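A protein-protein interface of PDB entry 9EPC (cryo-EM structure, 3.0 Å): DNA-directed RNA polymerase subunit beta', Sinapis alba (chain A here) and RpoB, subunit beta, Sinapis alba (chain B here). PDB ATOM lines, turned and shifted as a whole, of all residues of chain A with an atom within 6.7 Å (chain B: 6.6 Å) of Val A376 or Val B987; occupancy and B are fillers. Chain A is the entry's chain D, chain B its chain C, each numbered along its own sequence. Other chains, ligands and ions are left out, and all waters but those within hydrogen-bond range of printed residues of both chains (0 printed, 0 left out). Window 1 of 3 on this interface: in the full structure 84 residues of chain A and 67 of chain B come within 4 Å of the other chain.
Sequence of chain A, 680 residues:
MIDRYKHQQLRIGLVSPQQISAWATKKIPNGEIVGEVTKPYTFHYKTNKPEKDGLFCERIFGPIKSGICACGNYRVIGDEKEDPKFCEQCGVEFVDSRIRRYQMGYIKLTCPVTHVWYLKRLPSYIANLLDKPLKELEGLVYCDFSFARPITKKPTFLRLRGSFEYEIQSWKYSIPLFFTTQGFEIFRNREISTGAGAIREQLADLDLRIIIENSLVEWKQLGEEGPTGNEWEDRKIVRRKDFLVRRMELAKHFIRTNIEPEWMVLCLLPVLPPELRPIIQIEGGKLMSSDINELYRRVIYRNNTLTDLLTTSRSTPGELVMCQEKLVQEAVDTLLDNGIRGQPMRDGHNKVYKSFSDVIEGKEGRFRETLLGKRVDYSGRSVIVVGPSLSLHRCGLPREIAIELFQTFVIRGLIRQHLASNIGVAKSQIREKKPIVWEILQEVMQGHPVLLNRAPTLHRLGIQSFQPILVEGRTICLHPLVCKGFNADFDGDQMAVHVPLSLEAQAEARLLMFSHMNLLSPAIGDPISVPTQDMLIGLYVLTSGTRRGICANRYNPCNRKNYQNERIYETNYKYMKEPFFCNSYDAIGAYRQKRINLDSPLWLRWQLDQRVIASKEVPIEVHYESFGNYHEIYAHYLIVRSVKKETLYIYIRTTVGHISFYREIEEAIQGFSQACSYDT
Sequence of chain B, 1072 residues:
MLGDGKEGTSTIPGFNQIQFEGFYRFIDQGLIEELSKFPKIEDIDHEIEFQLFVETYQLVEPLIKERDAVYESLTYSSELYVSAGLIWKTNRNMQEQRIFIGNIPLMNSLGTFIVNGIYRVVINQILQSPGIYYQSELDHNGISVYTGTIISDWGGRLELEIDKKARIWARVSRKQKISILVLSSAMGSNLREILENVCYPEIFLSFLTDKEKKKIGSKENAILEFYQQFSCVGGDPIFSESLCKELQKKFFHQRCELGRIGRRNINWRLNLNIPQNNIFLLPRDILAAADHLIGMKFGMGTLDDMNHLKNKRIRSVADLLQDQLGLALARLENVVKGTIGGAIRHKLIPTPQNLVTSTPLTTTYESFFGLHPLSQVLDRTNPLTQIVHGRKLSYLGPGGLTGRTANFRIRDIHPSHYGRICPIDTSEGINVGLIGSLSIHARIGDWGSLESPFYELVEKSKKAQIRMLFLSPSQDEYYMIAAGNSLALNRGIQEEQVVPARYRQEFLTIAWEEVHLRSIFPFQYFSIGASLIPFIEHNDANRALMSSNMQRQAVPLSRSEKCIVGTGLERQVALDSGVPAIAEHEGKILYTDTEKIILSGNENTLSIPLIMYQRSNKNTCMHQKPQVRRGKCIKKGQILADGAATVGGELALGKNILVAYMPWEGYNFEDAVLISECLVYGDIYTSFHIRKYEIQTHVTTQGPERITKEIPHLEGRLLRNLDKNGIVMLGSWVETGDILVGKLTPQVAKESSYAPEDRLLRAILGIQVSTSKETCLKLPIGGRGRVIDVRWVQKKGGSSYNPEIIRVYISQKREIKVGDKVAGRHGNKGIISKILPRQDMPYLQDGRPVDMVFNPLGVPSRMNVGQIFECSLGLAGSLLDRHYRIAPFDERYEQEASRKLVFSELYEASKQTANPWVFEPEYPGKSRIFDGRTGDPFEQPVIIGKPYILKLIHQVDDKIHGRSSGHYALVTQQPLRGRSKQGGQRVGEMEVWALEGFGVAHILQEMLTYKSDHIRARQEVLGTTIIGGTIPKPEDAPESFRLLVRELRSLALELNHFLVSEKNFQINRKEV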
ATOM      1  N   GLU A 369      -4.748 -22.805  -2.368  1.00  0.00           N
ATOM      2  CA  GLU A 369      -3.901 -22.492  -1.221  1.00  0.00           C
ATOM      3  C   GLU A 369      -2.428 -22.448  -1.605  1.00  0.00           C
ATOM      4  O   GLU A 369      -1.693 -21.551  -1.178  1.00  0.00           O
ATOM      5  CB  GLU A 369      -4.135 -23.514  -0.108  1.00  0.00           C
ATOM      6  CG  GLU A 369      -3.293 -23.293   1.135  1.00  0.00           C
ATOM      7  CD  GLU A 369      -3.569 -24.322   2.212  1.00  0.00           C
ATOM      8  OE1 GLU A 369      -4.422 -25.205   1.987  1.00  0.00           O
ATOM      9  OE2 GLU A 369      -2.935 -24.247   3.286  1.00  0.00           O
ATOM     10  N   LEU A 372      -2.267 -19.469  -4.937  1.00  0.00           N
ATOM     11  CA  LEU A 372      -2.704 -18.148  -4.484  1.00  0.00           C
ATOM     12  C   LEU A 372      -2.259 -17.974  -3.034  1.00  0.00           C
ATOM     13  O   LEU A 372      -3.046 -18.053  -2.087  1.00  0.00           O
ATOM     14  CB  LEU A 372      -4.211 -17.987  -4.638  1.00  0.00           C
ATOM     15  CG  LEU A 372      -4.799 -17.936  -6.053  1.00  0.00           C
ATOM     16  CD1 LEU A 372      -3.979 -17.019  -6.948  1.00  0.00           C
ATOM     17  CD2 LEU A 372      -4.939 -19.324  -6.671  1.00  0.00           C
ATOM     18  N   GLY A 373      -0.962 -17.732  -2.866  1.00  0.00           N
ATOM     19  CA  GLY A 373      -0.382 -17.577  -1.547  1.00  0.00           C
ATOM     20  C   GLY A 373       0.745 -18.553  -1.286  1.00  0.00           C
ATOM     21  O   GLY A 373       0.751 -19.660  -1.833  1.00  0.00           O
ATOM     22  N   LYS A 374       1.704 -18.159  -0.452  1.00  0.00           N
ATOM     23  CA  LYS A 374       2.861 -18.990  -0.153  1.00  0.00           C
ATOM     24  C   LYS A 374       3.238 -18.834   1.312  1.00  0.00           C
ATOM     25  O   LYS A 374       2.884 -17.850   1.967  1.00  0.00           O
ATOM     26  CB  LYS A 374       4.066 -18.627  -1.031  1.00  0.00           C
ATOM     27  CG  LYS A 374       3.918 -18.981  -2.500  1.00  0.00           C
ATOM     28  CD  LYS A 374       3.849 -20.483  -2.704  1.00  0.00           C
ATOM     29  CE  LYS A 374       3.937 -20.834  -4.177  1.00  0.00           C
ATOM     30  NZ  LYS A 374       5.219 -20.380  -4.781  1.00  0.00           N
ATOM     31  N   ARG A 375       3.967 -19.828   1.822  1.00  0.00           N
ATOM     32  CA  ARG A 375       4.593 -19.739   3.140  1.00  0.00           C
ATOM     33  C   ARG A 375       5.897 -18.953   2.991  1.00  0.00           C
ATOM     34  O   ARG A 375       7.005 -19.493   3.017  1.00  0.00           O
ATOM     35  CB  ARG A 375       4.830 -21.127   3.719  1.00  0.00           C
ATOM     36  CG  ARG A 375       4.973 -21.151   5.230  1.00  0.00           C
ATOM     37  CD  ARG A 375       3.626 -20.959   5.905  1.00  0.00           C
ATOM     38  NE  ARG A 375       3.750 -20.794   7.348  1.00  0.00           N
ATOM     39  CZ  ARG A 375       2.722 -20.689   8.180  1.00  0.00           C
ATOM     40  NH1 ARG A 375       1.474 -20.745   7.747  1.00  0.00           N
ATOM     41  NH2 ARG A 375       2.954 -20.528   9.480  1.00  0.00           N
ATOM     42  N   VAL A 376       5.736 -17.640   2.828  1.00  0.00           N
ATOM     43  CA  VAL A 376       6.838 -16.783   2.405  1.00  0.00           C
ATOM     44  C   VAL A 376       7.884 -16.692   3.506  1.00  0.00           C
ATOM     45  O   VAL A 376       7.560 -16.469   4.681  1.00  0.00           O
ATOM     46  CB  VAL A 376       6.310 -15.395   2.016  1.00  0.00           C
ATOM     47  CG1 VAL A 376       7.454 -14.480   1.609  1.00  0.00           C
ATOM     48  CG2 VAL A 376       5.297 -15.517   0.891  1.00  0.00           C
ATOM     49  N   ASP A 377       9.150 -16.863   3.128  1.00  0.00           N
ATOM     50  CA  ASP A 377      10.255 -16.723   4.062  1.00  0.00           C
ATOM     51  C   ASP A 377      10.478 -15.248   4.394  1.00  0.00           C
ATOM     52  O   ASP A 377       9.765 -14.358   3.918  1.00  0.00           O
ATOM     53  CB  ASP A 377      11.522 -17.350   3.484  1.00  0.00           C
ATOM     54  CG  ASP A 377      11.356 -18.825   3.179  1.00  0.00           C
ATOM     55  OD1 ASP A 377      10.609 -19.506   3.913  1.00  0.00           O
ATOM     56  OD2 ASP A 377      11.972 -19.305   2.204  1.00  0.00           O
ATOM     57  N   TYR A 378      11.495 -14.991   5.219  1.00  0.00           N
ATOM     58  CA  TYR A 378      11.800 -13.643   5.700  1.00  0.00           C
ATOM     59  C   TYR A 378      10.576 -13.009   6.355  1.00  0.00           C
ATOM     60  O   TYR A 378      10.257 -11.840   6.132  1.00  0.00           O
ATOM     61  CB  TYR A 378      12.334 -12.757   4.572  1.00  0.00           C
ATOM     62  CG  TYR A 378      13.648 -13.221   3.989  1.00  0.00           C
ATOM     63  CD1 TYR A 378      13.684 -14.190   2.993  1.00  0.00           C
ATOM     64  CD2 TYR A 378      14.853 -12.687   4.427  1.00  0.00           C
ATOM     65  CE1 TYR A 378      14.883 -14.617   2.456  1.00  0.00           C
ATOM     66  CE2 TYR A 378      16.056 -13.108   3.895  1.00  0.00           C
ATOM     67  CZ  TYR A 378      16.065 -14.073   2.909  1.00  0.00           C
ATOM     68  OH  TYR A 378      17.260 -14.497   2.373  1.00  0.00           O
ATOM     69  N   SER A 379       9.878 -13.797   7.168  1.00  0.00           N
ATOM     70  CA  SER A 379       8.653 -13.365   7.822  1.00  0.00           C
ATOM     71  C   SER A 379       8.811 -13.460   9.333  1.00  0.00           C
ATOM     72  O   SER A 379       9.378 -14.427   9.850  1.00  0.00           O
ATOM     73  CB  SER A 379       7.458 -14.208   7.365  1.00  0.00           C
ATOM     74  OG  SER A 379       7.666 -15.583   7.636  1.00  0.00           O
ATOM     75  N   ASN A 453       2.184  -6.728   6.987  1.00  0.00           N
ATOM     76  CA  ASN A 453       0.957  -7.381   6.561  1.00  0.00           C
ATOM     77  C   ASN A 453       0.166  -7.848   7.773  1.00  0.00           C
ATOM     78  O   ASN A 453       0.723  -8.471   8.683  1.00  0.00           O
ATOM     79  CB  ASN A 453       1.260  -8.571   5.649  1.00  0.00           C
ATOM     80  CG  ASN A 453       0.030  -9.395   5.343  1.00  0.00           C
ATOM     81  OD1 ASN A 453      -1.081  -8.871   5.267  1.00  0.00           O
ATOM     82  ND2 ASN A 453       0.219 -10.697   5.171  1.00  0.00           N
ATOM     83  N   ILE A 463      -1.695  -4.653   3.653  1.00  0.00           N
ATOM     84  CA  ILE A 463      -0.263  -4.814   3.450  1.00  0.00           C
ATOM     85  C   ILE A 463       0.288  -3.486   2.954  1.00  0.00           C
ATOM     86  O   ILE A 463      -0.247  -2.898   2.007  1.00  0.00           O
ATOM     87  CB  ILE A 463       0.059  -5.959   2.471  1.00  0.00           C
ATOM     88  CG1 ILE A 463       1.555  -5.996   2.164  1.00  0.00           C
ATOM     89  CG2 ILE A 463      -0.752  -5.830   1.199  1.00  0.00           C
ATOM     90  CD1 ILE A 463       1.984  -7.222   1.400  1.00  0.00           C
ATOM     91  N   ALA A 496       2.626  -9.847  10.013  1.00  0.00           N
ATOM     92  CA  ALA A 496       3.683 -10.536   9.289  1.00  0.00           C
ATOM     93  C   ALA A 496       4.455  -9.518   8.464  1.00  0.00           C
ATOM     94  O   ALA A 496       3.859  -8.762   7.690  1.00  0.00           O
ATOM     95  CB  ALA A 496       3.112 -11.632   8.389  1.00  0.00           C
ATOM     96  N   HIS A 498       7.609  -8.710   5.784  1.00  0.00           N
ATOM     97  CA  HIS A 498       8.428  -9.276   4.723  1.00  0.00           C
ATOM     98  C   HIS A 498       9.394  -8.221   4.205  1.00  0.00           C
ATOM     99  O   HIS A 498       9.025  -7.054   4.041  1.00  0.00           O
ATOM    100  CB  HIS A 498       7.559  -9.798   3.580  1.00  0.00           C
ATOM    101  CG  HIS A 498       6.509 -10.768   4.020  1.00  0.00           C
ATOM    102  ND1 HIS A 498       6.723 -12.129   4.060  1.00  0.00           N
ATOM    103  CD2 HIS A 498       5.238 -10.573   4.446  1.00  0.00           C
ATOM    104  CE1 HIS A 498       5.626 -12.731   4.487  1.00  0.00           C
ATOM    105  NE2 HIS A 498       4.712 -11.810   4.728  1.00  0.00           N
ATOM    106  N   GLN B 985       5.807 -17.781   8.226  1.00  0.00           N
ATOM    107  CA  GLN B 985       4.443 -17.285   8.091  1.00  0.00           C
ATOM    108  C   GLN B 985       3.937 -17.478   6.666  1.00  0.00           C
ATOM    109  O   GLN B 985       4.721 -17.736   5.752  1.00  0.00           O
ATOM    110  CB  GLN B 985       4.367 -15.808   8.484  1.00  0.00           C
ATOM    111  CG  GLN B 985       4.947 -15.504   9.856  1.00  0.00           C
ATOM    112  CD  GLN B 985       4.212 -16.216  10.972  1.00  0.00           C
ATOM    113  OE1 GLN B 985       3.004 -16.443  10.892  1.00  0.00           O
ATOM    114  NE2 GLN B 985       4.939 -16.579  12.021  1.00  0.00           N
ATOM    115  N   ARG B 986       2.626 -17.351   6.478  1.00  0.00           N
ATOM    116  CA  ARG B 986       1.994 -17.552   5.183  1.00  0.00           C
ATOM    117  C   ARG B 986       1.350 -16.258   4.711  1.00  0.00           C
ATOM    118  O   ARG B 986       0.668 -15.578   5.486  1.00  0.00           O
ATOM    119  CB  ARG B 986       0.940 -18.662   5.240  1.00  0.00           C
ATOM    120  CG  ARG B 986       0.056 -18.713   4.007  1.00  0.00           C
ATOM    121  CD  ARG B 986      -0.873 -19.912   4.009  1.00  0.00           C
ATOM    122  NE  ARG B 986      -1.792 -19.864   2.878  1.00  0.00           N
ATOM    123  CZ  ARG B 986      -1.483 -20.242   1.645  1.00  0.00           C
ATOM    124  NH1 ARG B 986      -0.286 -20.720   1.348  1.00  0.00           N
ATOM    125  NH2 ARG B 986      -2.397 -20.133   0.685  1.00  0.00           N
ATOM    126  N   VAL B 987       1.568 -15.923   3.444  1.00  0.00           N
ATOM    127  CA  VAL B 987       0.856 -14.834   2.788  1.00  0.00           C
ATOM    128  C   VAL B 987      -0.411 -15.411   2.172  1.00  0.00           C
ATOM    129  O   VAL B 987      -0.350 -16.346   1.368  1.00  0.00           O
ATOM    130  CB  VAL B 987       1.733 -14.159   1.724  1.00  0.00           C
ATOM    131  CG1 VAL B 987       0.885 -13.302   0.804  1.00  0.00           C
ATOM    132  CG2 VAL B 987       2.812 -13.321   2.389  1.00  0.00           C
ATOM    133  N   GLY B 988      -1.562 -14.860   2.553  1.00  0.00           N
ATOM    134  CA  GLY B 988      -2.833 -15.369   2.088  1.00  0.00           C
ATOM    135  C   GLY B 988      -3.142 -14.955   0.664  1.00  0.00           C
ATOM    136  O   GLY B 988      -2.372 -14.270  -0.008  1.00  0.00           O
ATOM    137  N   GLU B 989      -4.310 -15.395   0.193  1.00  0.00           N
ATOM    138  CA  GLU B 989      -4.724 -15.075  -1.167  1.00  0.00           C
ATOM    139  C   GLU B 989      -5.168 -13.625  -1.302  1.00  0.00           C
ATOM    140  O   GLU B 989      -5.110 -13.066  -2.402  1.00  0.00           O
ATOM    141  CB  GLU B 989      -5.848 -16.012  -1.617  1.00  0.00           C
ATOM    142  CG  GLU B 989      -7.240 -15.612  -1.146  1.00  0.00           C
ATOM    143  CD  GLU B 989      -7.384 -15.633   0.363  1.00  0.00           C
ATOM    144  OE1 GLU B 989      -6.748 -16.489   1.013  1.00  0.00           O
ATOM    145  OE2 GLU B 989      -8.131 -14.788   0.900  1.00  0.00           O
ATOM    146  N   MET B 990      -5.609 -13.001  -0.207  1.00  0.00           N
ATOM    147  CA  MET B 990      -6.059 -11.618  -0.292  1.00  0.00           C
ATOM    148  C   MET B 990      -4.893 -10.652  -0.445  1.00  0.00           C
ATOM    149  O   MET B 990      -5.017  -9.640  -1.143  1.00  0.00           O
ATOM    150  CB  MET B 990      -6.888 -11.253   0.936  1.00  0.00           C
ATOM    151  CG  MET B 990      -7.399  -9.829   0.901  1.00  0.00           C
ATOM    152  SD  MET B 990      -8.349  -9.358   2.351  1.00  0.00           S
ATOM    153  CE  MET B 990      -8.644  -7.634   1.973  1.00  0.00           C
ATOM    154  N   GLU B 991      -3.757 -10.944   0.194  1.00  0.00           N
ATOM    155  CA  GLU B 991      -2.589 -10.083   0.046  1.00  0.00           C
ATOM    156  C   GLU B 991      -2.131 -10.013  -1.403  1.00  0.00           C
ATOM    157  O   GLU B 991      -1.568  -8.999  -1.827  1.00  0.00           O
ATOM    158  CB  GLU B 991      -1.452 -10.577   0.939  1.00  0.00           C
ATOM    159  CG  GLU B 991      -1.687 -10.394   2.429  1.00  0.00           C
ATOM    160  CD  GLU B 991      -2.632 -11.426   3.019  1.00  0.00           C
ATOM    161  OE1 GLU B 991      -3.198 -12.233   2.252  1.00  0.00           O
ATOM    162  OE2 GLU B 991      -2.810 -11.429   4.255  1.00  0.00           O
ATOM    163  N   VAL B 992      -2.361 -11.078  -2.172  1.00  0.00           N
ATOM    164  CA  VAL B 992      -2.061 -11.044  -3.599  1.00  0.00           C
ATOM    165  C   VAL B 992      -2.914  -9.993  -4.293  1.00  0.00           C
ATOM    166  O   VAL B 992      -2.429  -9.240  -5.145  1.00  0.00           O
ATOM    167  CB  VAL B 992      -2.259 -12.439  -4.217  1.00  0.00           C
ATOM    168  CG1 VAL B 992      -2.074 -12.385  -5.722  1.00  0.00           C
ATOM    169  CG2 VAL B 992      -1.294 -13.430  -3.593  1.00  0.00           C
ATOM    170  N   LEU B 995      -1.521  -6.536  -3.422  1.00  0.00           N
ATOM    171  CA  LEU B 995      -0.285  -6.261  -4.145  1.00  0.00           C
ATOM    172  C   LEU B 995      -0.562  -5.951  -5.609  1.00  0.00           C
ATOM    173  O   LEU B 995       0.048  -5.045  -6.187  1.00  0.00           O
ATOM    174  CB  LEU B 995       0.672  -7.445  -4.017  1.00  0.00           C
ATOM    175  CG  LEU B 995       1.264  -7.670  -2.627  1.00  0.00           C
ATOM    176  CD1 LEU B 995       2.159  -8.895  -2.619  1.00  0.00           C
ATOM    177  CD2 LEU B 995       2.031  -6.445  -2.177  1.00  0.00           C
ATOM    178  N   GLU B1006       8.148 -11.890  -5.979  1.00  0.00           N
ATOM    179  CA  GLU B1006       9.098 -12.260  -4.935  1.00  0.00           C
ATOM    180  C   GLU B1006       8.438 -13.114  -3.860  1.00  0.00           C
ATOM    181  O   GLU B1006       9.082 -13.990  -3.270  1.00  0.00           O
ATOM    182  CB  GLU B1006       9.726 -11.007  -4.328  1.00  0.00           C
ATOM    183  CG  GLU B1006      10.808 -11.303  -3.310  1.00  0.00           C
ATOM    184  CD  GLU B1006      11.770 -10.151  -3.133  1.00  0.00           C
ATOM    185  OE1 GLU B1006      12.055  -9.458  -4.132  1.00  0.00           O
ATOM    186  OE2 GLU B1006      12.242  -9.936  -1.998  1.00  0.00           O
ATOM    187  N   MET B1007       7.152 -12.880  -3.593  1.00  0.00           N
ATOM    188  CA  MET B1007       6.436 -13.703  -2.622  1.00  0.00           C
ATOM    189  C   MET B1007       6.335 -15.152  -3.088  1.00  0.00           C
ATOM    190  O   MET B1007       6.497 -16.081  -2.289  1.00  0.00           O
ATOM    191  CB  MET B1007       5.043 -13.129  -2.371  1.00  0.00           C
ATOM    192  CG  MET B1007       5.019 -11.650  -2.023  1.00  0.00           C
ATOM    193  SD  MET B1007       6.146 -11.194  -0.698  1.00  0.00           S
ATOM    194  CE  MET B1007       5.002 -10.471   0.472  1.00  0.00           C
ATOM    195  N   LEU B1008       6.069 -15.364  -4.376  1.00  0.00           N
ATOM    196  CA  LEU B1008       5.840 -16.692  -4.928  1.00  0.00           C
ATOM    197  C   LEU B1008       7.096 -17.295  -5.550  1.00  0.00           C
ATOM    198  O   LEU B1008       6.995 -18.091  -6.490  1.00  0.00           O
ATOM    199  CB  LEU B1008       4.715 -16.634  -5.962  1.00  0.00           C
ATOM    200  CG  LEU B1008       3.594 -15.641  -5.645  1.00  0.00           C
ATOM    201  CD1 LEU B1008       2.633 -15.534  -6.814  1.00  0.00           C
ATOM    202  CD2 LEU B1008       2.853 -16.033  -4.376  1.00  0.00           C
ATOM    203  N   LYS B1011      11.747 -16.605  -2.019  1.00  0.00           N
ATOM    204  CA  LYS B1011      11.220 -16.439  -0.669  1.00  0.00           C
ATOM    205  C   LYS B1011       9.982 -17.308  -0.486  1.00  0.00           C
ATOM    206  O   LYS B1011       8.940 -16.836  -0.022  1.00  0.00           O
ATOM    207  CB  LYS B1011      10.885 -14.973  -0.390  1.00  0.00           C
ATOM    208  CG  LYS B1011      12.094 -14.062  -0.301  1.00  0.00           C
ATOM    209  CD  LYS B1011      11.675 -12.624  -0.043  1.00  0.00           C
ATOM    210  CE  LYS B1011      10.809 -12.512   1.201  1.00  0.00           C
ATOM    211  NZ  LYS B1011      10.355 -11.113   1.436  1.00  0.00           N
ATOM    212  N   SER B1012      10.100 -18.583  -0.854  1.00  0.00           N
ATOM    213  CA  SER B1012       9.037 -19.576  -0.745  1.00  0.00           C
ATOM    214  C   SER B1012       9.626 -20.947  -1.046  1.00  0.00           C
ATOM    215  O   SER B1012      10.850 -21.110  -1.058  1.00  0.00           O
ATOM    216  CB  SER B1012       7.873 -19.267  -1.689  1.00  0.00           C
ATOM    217  OG  SER B1012       6.875 -20.269  -1.606  1.00  0.00           O
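The backbone carbonyl oxygen (O) of Gln B985 is in hydrogen-bond range of the backbone NH (N) of Val A376.
The backbone NH (N) of Gln B985 lies within hydrogen-bond range of the side-chain hydroxyl (OG) of Ser A379, 2.9 Å away.
O of Glu A369 sits at hydrogen-bond distance from NH2 of Arg B986 (2.4 Å).
N of Val B987 is in hydrogen-bond range of O of Lys A374, 2.8 Å away.
ND2 of Asn A453 lies within hydrogen-bond range of OE2 of Glu B991, at 3.2 Å.
The side-chain amino group of Lys A374 sits at hydrogen-bond distance from the backbone carbonyl oxygen of Leu B1008 (3.4 Å).
The backbone carbonyl oxygen (O) of Lys B1011 lies within hydrogen-bond range of the backbone NH (N) of Asp A377, 3.2 Å away.
The backbone NH (N) of Gly B988 sits at hydrogen-bond distance from the side-chain carboxylate (OE1) of Glu B991 (3.1 Å).
O of Val A376 sits at hydrogen-bond distance from OG of Ser A379 (3.1 Å).
The backbone carbonyl oxygen (O) of Asn A453 is in hydrogen-bond range of the backbone NH (N) of Ala A496.
Among the printed residues, pairs that only touch across the chains: Leu A372 with Arg B986 (3.5 Å), Leu A372 with Glu B989 (3.5 Å), Gly A373 with Arg B986 (3.5 Å), Gly A373 with Val B987 (3.2 Å), Lys A374 with Arg B986 (3.4 Å), Lys A374 with Met B1007 (3.7 Å), Lys A374 with Ser B1012 (3.2 Å), Arg A375 with Gln B985 (3.2 Å), Arg A375 with Arg B986 (3.3 Å), Val A376 with Val B987 (3.6 Å), Val A376 with Met B1007 (3.4 Å), Val A376 with Lys B1011 (3.2 Å), Asp A377 with Ser B1012 (3.7 Å), Tyr A378 with Lys B1011 (3.7 Å), Ile A463 with Leu B995 (3.7 Å), His A498 with Val B987 (3.4 Å), His A498 with Met B1007 (3.9 Å) and His A498 with Lys B1011 (3.8 Å).
Of the printed residues of chain B, Val A376 touches Gln B985, Val B987, Met B1007 and Lys B1011.
Val B987 touches four residues of chain A.
Of the printed residues of chain A, Arg B986 touches Glu A369, Leu A372, Gly A373, Lys A374 and Arg A375.
Printed residues of chain B within 4 Å of Ser A379: Gln B985 (2.9 Å).
Of the printed residues of chain B, Asp A377 touches Lys B1011 (3.2 Å) and Ser B1012 (3.7 Å).
Of the printed residues of chain B, Ile A463 touches Leu B995 (3.7 Å).
Printed residues of chain B within 4 Å of Lys A374: Arg B986, Val B987, Met B1007, Leu B1008 and Ser B1012.
Val B992 touches none of the printed residues of chain A.
Ala A496 touches none of the printed residues of chain B.
The nearest residue of chain B that does not touch Val A376 is Arg B986 (4.4 Å).
The nearest printed residue of chain A that does not touch Ser B1012 is Arg A375 (4.3 Å).
Of the 14 printed residues of chain B, 10 touch a printed residue of chain A.
Printed residues of chain A that touch a printed residue of chain B: Glu A369, Leu A372, Gly A373, Lys A374, Arg A375, Val A376, Asp A377, Tyr A378, Ser A379, Asn A453, Ile A463 and His A498.
Hydrophobic or aromatic side chains of chain A within 4 Å of the printed part of chain B: Leu A372, Val A376, Tyr A378, Ile A463 and His A498.
Among the printed residues, no Asp or Glu carboxylate lies within 4 Å of a Lys or Arg side-chain nitrogen of the other chain.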
